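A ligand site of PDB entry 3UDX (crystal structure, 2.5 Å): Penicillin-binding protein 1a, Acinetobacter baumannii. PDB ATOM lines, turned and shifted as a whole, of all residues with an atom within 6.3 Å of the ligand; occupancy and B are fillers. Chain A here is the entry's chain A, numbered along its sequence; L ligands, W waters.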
ATOM      1  N   PRO A 424       5.706  14.701 -36.997  1.00  0.00           N
ATOM      2  CA  PRO A 424       6.030  14.953 -35.579  1.00  0.00           C
ATOM      3  C   PRO A 424       4.957  14.539 -34.578  1.00  0.00           C
ATOM      4  O   PRO A 424       5.276  14.302 -33.414  1.00  0.00           O
ATOM      5  CB  PRO A 424       6.307  16.457 -35.527  1.00  0.00           C
ATOM      6  CG  PRO A 424       5.597  17.033 -36.696  1.00  0.00           C
ATOM      7  CD  PRO A 424       5.316  15.946 -37.703  1.00  0.00           C
ATOM      8  N   GLY A 425       3.716  14.442 -35.032  1.00  0.00           N
ATOM      9  CA  GLY A 425       2.594  14.128 -34.151  1.00  0.00           C
ATOM     10  C   GLY A 425       2.397  15.233 -33.118  1.00  0.00           C
ATOM     11  O   GLY A 425       2.457  16.434 -33.435  1.00  0.00           O
ATOM     12  N   SER A 426       2.255  14.822 -31.857  1.00  0.00           N
ATOM     13  CA  SER A 426       2.006  15.682 -30.703  1.00  0.00           C
ATOM     14  C   SER A 426       3.109  16.674 -30.404  1.00  0.00           C
ATOM     15  O   SER A 426       2.856  17.652 -29.694  1.00  0.00           O
ATOM     16  CB  SER A 426       1.704  14.857 -29.465  1.00  0.00           C
ATOM     17  OG  SER A 426       0.492  14.163 -29.618  1.00  0.00           O
ATOM     18  N   THR A 427       4.333  16.464 -30.941  1.00  0.00           N
ATOM     19  CA  THR A 427       5.445  17.396 -30.724  1.00  0.00           C
ATOM     20  C   THR A 427       5.244  18.745 -31.435  1.00  0.00           C
ATOM     21  O   THR A 427       5.910  19.719 -31.077  1.00  0.00           O
ATOM     22  CB  THR A 427       6.822  16.744 -30.941  1.00  0.00           C
ATOM     23  OG1 THR A 427       6.861  16.200 -32.250  1.00  0.00           O
ATOM     24  CG2 THR A 427       7.142  15.679 -29.914  1.00  0.00           C
ATOM     25  N   LYS A 429       2.150  20.215 -31.395  1.00  0.00           N
ATOM     26  CA  LYS A 429       1.096  20.812 -30.569  1.00  0.00           C
ATOM     27  C   LYS A 429       1.520  22.044 -29.761  1.00  0.00           C
ATOM     28  O   LYS A 429       0.770  23.033 -29.809  1.00  0.00           O
ATOM     29  CB  LYS A 429       0.372  19.780 -29.676  1.00  0.00           C
ATOM     30  CG  LYS A 429      -0.504  18.798 -30.446  1.00  0.00           C
ATOM     31  CD  LYS A 429      -1.419  18.011 -29.522  1.00  0.00           C
ATOM     32  CE  LYS A 429      -2.078  16.846 -30.227  1.00  0.00           C
ATOM     33  NZ  LYS A 429      -2.945  17.281 -31.350  1.00  0.00           N
ATOM     34  N   LYS A 460     -10.628  12.072 -34.302  1.00  0.00           N
ATOM     35  CA  LYS A 460     -10.862  11.311 -33.089  1.00  0.00           C
ATOM     36  C   LYS A 460      -9.650  11.353 -32.180  1.00  0.00           C
ATOM     37  O   LYS A 460      -8.530  11.573 -32.637  1.00  0.00           O
ATOM     38  CB  LYS A 460     -11.285   9.867 -33.413  1.00  0.00           C
ATOM     39  CG  LYS A 460     -12.778   9.741 -33.710  1.00  0.00           C
ATOM     40  CD  LYS A 460     -13.088   8.841 -34.888  1.00  0.00           C
ATOM     41  CE  LYS A 460     -14.556   8.874 -35.248  1.00  0.00           C
ATOM     42  NZ  LYS A 460     -14.894   7.899 -36.317  1.00  0.00           N
ATOM     43  N   ASN A 461      -9.886  11.172 -30.875  1.00  0.00           N
ATOM     44  CA  ASN A 461      -8.825  11.120 -29.880  1.00  0.00           C
ATOM     45  C   ASN A 461      -8.249   9.711 -29.931  1.00  0.00           C
ATOM     46  O   ASN A 461      -9.009   8.754 -30.044  1.00  0.00           O
ATOM     47  CB  ASN A 461      -9.380  11.468 -28.478  1.00  0.00           C
ATOM     48  CG  ASN A 461      -9.675  12.951 -28.269  1.00  0.00           C
ATOM     49  OD1 ASN A 461      -9.057  13.847 -28.858  1.00  0.00           O
ATOM     50  ND2 ASN A 461     -10.588  13.238 -27.371  1.00  0.00           N
ATOM     51  N   SER A 462      -6.907   9.596 -29.900  1.00  0.00           N
ATOM     52  CA  SER A 462      -6.206   8.316 -29.984  1.00  0.00           C
ATOM     53  C   SER A 462      -6.775   7.197 -29.065  1.00  0.00           C
ATOM     54  O   SER A 462      -6.905   6.051 -29.500  1.00  0.00           O
ATOM     55  CB  SER A 462      -4.709   8.505 -29.790  1.00  0.00           C
ATOM     56  OG  SER A 462      -4.043   8.654 -31.043  1.00  0.00           O
ATOM     57  N   ASP A 463      -7.154   7.562 -27.831  1.00  0.00           N
ATOM     58  CA  ASP A 463      -7.713   6.625 -26.859  1.00  0.00           C
ATOM     59  C   ASP A 463      -9.246   6.407 -26.992  1.00  0.00           C
ATOM     60  O   ASP A 463      -9.812   5.634 -26.212  1.00  0.00           O
ATOM     61  CB  ASP A 463      -7.330   7.054 -25.426  1.00  0.00           C
ATOM     62  CG  ASP A 463      -7.698   8.476 -25.029  1.00  0.00           C
ATOM     63  OD1 ASP A 463      -8.391   9.173 -25.816  1.00  0.00           O
ATOM     64  OD2 ASP A 463      -7.317   8.891 -23.904  1.00  0.00           O
ATOM     65  N   GLY A 464      -9.891   7.100 -27.920  1.00  0.00           N
ATOM     66  CA  GLY A 464     -11.343   7.032 -28.096  1.00  0.00           C
ATOM     67  C   GLY A 464     -12.094   7.539 -26.857  1.00  0.00           C
ATOM     68  O   GLY A 464     -13.214   7.103 -26.586  1.00  0.00           O
ATOM     69  N   TYR A 477      -0.970  18.450 -22.378  1.00  0.00           N
ATOM     70  CA  TYR A 477      -0.334  17.333 -21.697  1.00  0.00           C
ATOM     71  C   TYR A 477      -0.930  16.013 -22.153  1.00  0.00           C
ATOM     72  O   TYR A 477      -0.187  15.102 -22.499  1.00  0.00           O
ATOM     73  CB  TYR A 477      -0.430  17.474 -20.150  1.00  0.00           C
ATOM     74  CG  TYR A 477       0.036  16.239 -19.410  1.00  0.00           C
ATOM     75  CD1 TYR A 477       1.358  15.804 -19.474  1.00  0.00           C
ATOM     76  CD2 TYR A 477      -0.872  15.464 -18.674  1.00  0.00           C
ATOM     77  CE1 TYR A 477       1.775  14.653 -18.815  1.00  0.00           C
ATOM     78  CE2 TYR A 477      -0.457  14.304 -18.003  1.00  0.00           C
ATOM     79  CZ  TYR A 477       0.871  13.906 -18.077  1.00  0.00           C
ATOM     80  OH  TYR A 477       1.285  12.763 -17.445  1.00  0.00           O
ATOM     81  N   LEU A 478      -2.249  15.917 -22.182  1.00  0.00           N
ATOM     82  CA  LEU A 478      -2.927  14.698 -22.593  1.00  0.00           C
ATOM     83  C   LEU A 478      -3.056  14.506 -24.113  1.00  0.00           C
ATOM     84  O   LEU A 478      -3.497  13.436 -24.544  1.00  0.00           O
ATOM     85  CB  LEU A 478      -4.251  14.521 -21.840  1.00  0.00           C
ATOM     86  CG  LEU A 478      -4.116  14.418 -20.316  1.00  0.00           C
ATOM     87  CD1 LEU A 478      -5.450  14.604 -19.625  1.00  0.00           C
ATOM     88  CD2 LEU A 478      -3.418  13.118 -19.901  1.00  0.00           C
ATOM     89  N   SER A 479      -2.649  15.522 -24.902  1.00  0.00           N
ATOM     90  CA  SER A 479      -2.656  15.561 -26.372  1.00  0.00           C
ATOM     91  C   SER A 479      -4.058  15.373 -26.978  1.00  0.00           C
ATOM     92  O   SER A 479      -4.300  14.458 -27.754  1.00  0.00           O
ATOM     93  CB  SER A 479      -1.620  14.600 -26.954  1.00  0.00           C
ATOM     94  OG  SER A 479      -0.316  15.026 -26.615  1.00  0.00           O
ATOM     95  N   ASN A 481      -6.611  15.836 -29.520  1.00  0.00           N
ATOM     96  CA  ASN A 481      -6.765  16.191 -30.939  1.00  0.00           C
ATOM     97  C   ASN A 481      -7.960  17.074 -31.200  1.00  0.00           C
ATOM     98  O   ASN A 481      -7.868  18.011 -31.994  1.00  0.00           O
ATOM     99  CB  ASN A 481      -6.821  14.966 -31.825  1.00  0.00           C
ATOM    100  CG  ASN A 481      -5.573  14.106 -31.805  1.00  0.00           C
ATOM    101  OD1 ASN A 481      -4.466  14.587 -31.562  1.00  0.00           O
ATOM    102  ND2 ASN A 481      -5.728  12.826 -32.126  1.00  0.00           N
ATOM    103  N   ALA A 517      -2.832  20.368 -37.107  1.00  0.00           N
ATOM    104  CA  ALA A 517      -3.125  20.343 -35.673  1.00  0.00           C
ATOM    105  C   ALA A 517      -2.806  18.958 -35.072  1.00  0.00           C
ATOM    106  O   ALA A 517      -2.492  18.863 -33.892  1.00  0.00           O
ATOM    107  CB  ALA A 517      -4.588  20.657 -35.462  1.00  0.00           C
ATOM    108  N   LEU A 518      -2.915  17.891 -35.877  1.00  0.00           N
ATOM    109  CA  LEU A 518      -2.649  16.505 -35.472  1.00  0.00           C
ATOM    110  C   LEU A 518      -1.224  16.032 -35.785  1.00  0.00           C
ATOM    111  O   LEU A 518      -0.918  14.860 -35.549  1.00  0.00           O
ATOM    112  CB  LEU A 518      -3.696  15.566 -36.111  1.00  0.00           C
ATOM    113  CG  LEU A 518      -4.959  15.304 -35.294  1.00  0.00           C
ATOM    114  CD1 LEU A 518      -5.853  16.526 -35.235  1.00  0.00           C
ATOM    115  CD2 LEU A 518      -5.735  14.122 -35.848  1.00  0.00           C
ATOM    116  N   GLY A 519      -0.383  16.935 -36.285  1.00  0.00           N
ATOM    117  CA  GLY A 519       1.036  16.682 -36.573  1.00  0.00           C
ATOM    118  C   GLY A 519       1.311  15.784 -37.757  1.00  0.00           C
ATOM    119  O   GLY A 519       2.238  14.974 -37.727  1.00  0.00           O
ATOM    120  N   LYS A 661       8.257  17.781 -24.399  1.00  0.00           N
ATOM    121  CA  LYS A 661       7.038  17.177 -24.920  1.00  0.00           C
ATOM    122  C   LYS A 661       7.349  15.873 -25.674  1.00  0.00           C
ATOM    123  O   LYS A 661       8.264  15.845 -26.504  1.00  0.00           O
ATOM    124  CB  LYS A 661       6.283  18.183 -25.820  1.00  0.00           C
ATOM    125  CG  LYS A 661       4.974  17.691 -26.442  1.00  0.00           C
ATOM    126  CD  LYS A 661       3.758  17.896 -25.540  1.00  0.00           C
ATOM    127  CE  LYS A 661       2.467  17.395 -26.174  1.00  0.00           C
ATOM    128  NZ  LYS A 661       2.395  15.918 -26.280  1.00  0.00           N
ATOM    129  N   THR A 662       6.565  14.826 -25.380  1.00  0.00           N
ATOM    130  CA  THR A 662       6.619  13.521 -26.046  1.00  0.00           C
ATOM    131  C   THR A 662       5.725  13.568 -27.292  1.00  0.00           C
ATOM    132  O   THR A 662       4.792  14.404 -27.366  1.00  0.00           O
ATOM    133  CB  THR A 662       6.053  12.411 -25.139  1.00  0.00           C
ATOM    134  OG1 THR A 662       4.730  12.766 -24.751  1.00  0.00           O
ATOM    135  CG2 THR A 662       6.909  12.107 -23.939  1.00  0.00           C
ATOM    136  N   GLY A 663       5.965  12.621 -28.206  1.00  0.00           N
ATOM    137  CA  GLY A 663       5.167  12.409 -29.404  1.00  0.00           C
ATOM    138  C   GLY A 663       5.089  10.944 -29.785  1.00  0.00           C
ATOM    139  O   GLY A 663       6.051  10.197 -29.614  1.00  0.00           O
ATOM    140  N   THR A 664       3.908  10.510 -30.256  1.00  0.00           N
ATOM    141  CA  THR A 664       3.655   9.157 -30.769  1.00  0.00           C
ATOM    142  C   THR A 664       2.652   9.268 -31.912  1.00  0.00           C
ATOM    143  O   THR A 664       1.454   9.494 -31.651  1.00  0.00           O
ATOM    144  CB  THR A 664       3.086   8.173 -29.727  1.00  0.00           C
ATOM    145  OG1 THR A 664       3.695   8.361 -28.437  1.00  0.00           O
ATOM    146  CG2 THR A 664       3.209   6.730 -30.191  1.00  0.00           C
ATOM    147  N   THR A 665       3.134   9.091 -33.161  1.00  0.00           N
ATOM    148  CA  THR A 665       2.296   9.142 -34.362  1.00  0.00           C
ATOM    149  C   THR A 665       1.347   7.946 -34.387  1.00  0.00           C
ATOM    150  O   THR A 665       1.489   7.027 -33.573  1.00  0.00           O
ATOM    151  CB  THR A 665       3.147   9.305 -35.647  1.00  0.00           C
ATOM    152  OG1 THR A 665       3.983   8.170 -35.819  1.00  0.00           O
ATOM    153  CG2 THR A 665       3.968  10.576 -35.650  1.00  0.00           C
ATOM    154  N   ASN A 666       0.357   7.948 -35.311  1.00  0.00           N
ATOM    155  CA  ASN A 666      -0.619   6.867 -35.401  1.00  0.00           C
ATOM    156  C   ASN A 666      -0.001   5.522 -35.728  1.00  0.00           C
ATOM    157  O   ASN A 666       0.876   5.410 -36.610  1.00  0.00           O
ATOM    158  CB  ASN A 666      -1.796   7.221 -36.307  1.00  0.00           C
ATOM    159  CG  ASN A 666      -2.438   8.532 -35.948  1.00  0.00           C
ATOM    160  OD1 ASN A 666      -2.146   9.558 -36.559  1.00  0.00           O
ATOM    161  ND2 ASN A 666      -3.281   8.536 -34.918  1.00  0.00           N
ATOM    162  N   TRP A 672       8.791  10.274 -30.367  1.00  0.00           N
ATOM    163  CA  TRP A 672       9.552  11.521 -30.302  1.00  0.00           C
ATOM    164  C   TRP A 672       9.634  12.085 -28.910  1.00  0.00           C
ATOM    165  O   TRP A 672       8.675  12.016 -28.150  1.00  0.00           O
ATOM    166  CB  TRP A 672       8.864  12.626 -31.126  1.00  0.00           C
ATOM    167  CG  TRP A 672       8.740  12.481 -32.607  1.00  0.00           C
ATOM    168  CD1 TRP A 672       7.690  11.930 -33.289  1.00  0.00           C
ATOM    169  CD2 TRP A 672       9.547  13.137 -33.599  1.00  0.00           C
ATOM    170  NE1 TRP A 672       7.842  12.118 -34.636  1.00  0.00           N
ATOM    171  CE2 TRP A 672       8.957  12.887 -34.859  1.00  0.00           C
ATOM    172  CE3 TRP A 672      10.748  13.876 -33.547  1.00  0.00           C
ATOM    173  CZ2 TRP A 672       9.498  13.378 -36.059  1.00  0.00           C
ATOM    174  CZ3 TRP A 672      11.291  14.351 -34.732  1.00  0.00           C
ATOM    175  CH2 TRP A 672      10.656  14.127 -35.965  1.00  0.00           C
ATOM    176  N   TYR A 699       5.476   4.169 -26.840  1.00  0.00           N
ATOM    177  CA  TYR A 699       5.111   5.586 -26.890  1.00  0.00           C
ATOM    178  C   TYR A 699       6.404   6.392 -26.754  1.00  0.00           C
ATOM    179  O   TYR A 699       7.368   5.870 -26.204  1.00  0.00           O
ATOM    180  CB  TYR A 699       4.167   5.966 -25.737  1.00  0.00           C
ATOM    181  CG  TYR A 699       2.935   5.107 -25.540  1.00  0.00           C
ATOM    182  CD1 TYR A 699       1.891   5.138 -26.470  1.00  0.00           C
ATOM    183  CD2 TYR A 699       2.753   4.364 -24.376  1.00  0.00           C
ATOM    184  CE1 TYR A 699       0.732   4.377 -26.282  1.00  0.00           C
ATOM    185  CE2 TYR A 699       1.599   3.601 -24.172  1.00  0.00           C
ATOM    186  CZ  TYR A 699       0.589   3.615 -25.125  1.00  0.00           C
ATOM    187  OH  TYR A 699      -0.547   2.864 -24.919  1.00  0.00           O
ATOM    188  N   GLY A 700       6.380   7.656 -27.204  1.00  0.00           N
ATOM    189  CA  GLY A 700       7.496   8.597 -27.125  1.00  0.00           C
ATOM    190  C   GLY A 700       8.183   8.571 -25.777  1.00  0.00           C
ATOM    191  O   GLY A 700       9.419   8.461 -25.716  1.00  0.00           O
ATOM    192  N   GLY A 701       7.370   8.597 -24.711  1.00  0.00           N
ATOM    193  CA  GLY A 701       7.799   8.536 -23.312  1.00  0.00           C
ATOM    194  C   GLY A 701       8.555   7.272 -22.915  1.00  0.00           C
ATOM    195  O   GLY A 701       9.342   7.295 -21.963  1.00  0.00           O
HETATM  196  C1  LIG L   1       0.706  12.671 -30.161  1.00  0.00           C
HETATM  197  C2  LIG L   1      -0.213   9.562 -27.603  1.00  0.00           C
HETATM  198  C3  LIG L   1      -0.608  11.893 -30.161  1.00  0.00           C
HETATM  199  C4  LIG L   1      -1.003  11.447 -28.755  1.00  0.00           C
HETATM  200  C5  LIG L   1       0.606  10.580 -27.355  1.00  0.00           C
HETATM  201  O1  LIG L   1       1.720  12.173 -30.586  1.00  0.00           O
HETATM  202  C6  LIG L   1      -1.773  12.656 -30.804  1.00  0.00           C
HETATM  203  O2  LIG L   1      -2.761  11.687 -31.138  1.00  0.00           O
HETATM  204  C7  LIG L   1      -1.442  13.479 -32.056  1.00  0.00           C
HETATM  205  N1  LIG L   1       0.049  11.699 -27.792  1.00  0.00           N
HETATM  206  C8  LIG L   1       1.992  10.606 -26.858  1.00  0.00           C
HETATM  207  O3  LIG L   1       2.629  11.686 -26.938  1.00  0.00           O
HETATM  208  O4  LIG L   1       2.542   9.578 -26.379  1.00  0.00           O
HETATM  209  S1  LIG L   1      -0.238   8.063 -26.863  1.00  0.00           S
HETATM  210  C9  LIG L   1      -1.699   7.880 -25.886  1.00  0.00           C
HETATM  211  C10 LIG L   1      -2.278   6.472 -26.031  1.00  0.00           C
HETATM  212  N2  LIG L   1      -3.306   6.365 -27.057  1.00  0.00           N
HETATM  213  C11 LIG L   1      -3.809   5.182 -27.392  1.00  0.00           C
HETATM  214  N3  LIG L   1      -4.804   4.698 -26.775  1.00  0.00           N
HETATM  215  C12 LIG L   1      -1.232   9.940 -28.640  1.00  0.00           C
HETATM  216  O   HOH W   1      -1.497   9.057 -32.106  1.00  0.00           O
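The backbone NH (N) of Thr 664 lies within hydrogen-bond range of an oxygen (O1) of the ligand, 2.8 Å away.
O2 of the ligand sits at hydrogen-bond distance from OG of Ser 462 (3.3 Å).
OG of Ser 426 is bonded to C1 of the ligand (1.6 Å).
An oxygen (O4) of the ligand lies within hydrogen-bond range of the side-chain hydroxyl of Thr 664 (2.7 Å).
OG1 of Thr 662 lies within hydrogen-bond range of O3 of the ligand.
The side-chain amide nitrogen (ND2) of Asn 481 lies within hydrogen-bond range of an oxygen (O2) of the ligand.
An oxygen (O1) of the ligand sits close to the backbone NH of Ser 426, at 3.0 Å.
The side-chain hydroxyl (OG1) of Thr 664 is in hydrogen-bond range of the backbone NH (N) of Gly 700 (3.0 Å).
The side-chain hydroxyl (OG) of Ser 479 is in hydrogen-bond range of the side-chain amino group (NZ) of Lys 661 (2.9 Å).
N of Gly 663 lies within hydrogen-bond range of O of Trp 672, 2.8 Å away.
The side-chain amide oxygen (OD1) of Asn 481 sits at hydrogen-bond distance from the side-chain amino group (NZ) of Lys 429.
The backbone NH (N) of Asn 481 is in hydrogen-bond range of the side-chain amide oxygen (OD1) of Asn 461 (3.2 Å).
O of Lys 460 sits at hydrogen-bond distance from ND2 of Asn 481.
The side-chain hydroxyl (OG) of Ser 479 is in hydrogen-bond range of the side-chain hydroxyl (OG) of Ser 426, 3.2 Å away.
The backbone carbonyl oxygen (O) of Ala 517 sits at hydrogen-bond distance from the side-chain amino group (NZ) of Lys 429 (3.0 Å).
CE of Lys 429 touches C7 of the ligand, 3.9 Å away.
CA of Asp 463 touches N3 of the ligand, at 3.5 Å.
Ser 479 touches the ligand (CB to N1, 3.5 Å).
Leu 518 touches the ligand.
Gly 663 touches the ligand (CA to O3, 3.6 Å).
CD1 of Tyr 699 touches S1 of the ligand, 3.6 Å away.
Water W1 lies within hydrogen-bond range of OG of Ser 462 (2.8 Å), O of Thr 664 (3.0 Å), O2 of the ligand (3.1 Å) and ND2 of Asn 666 (3.4 Å).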
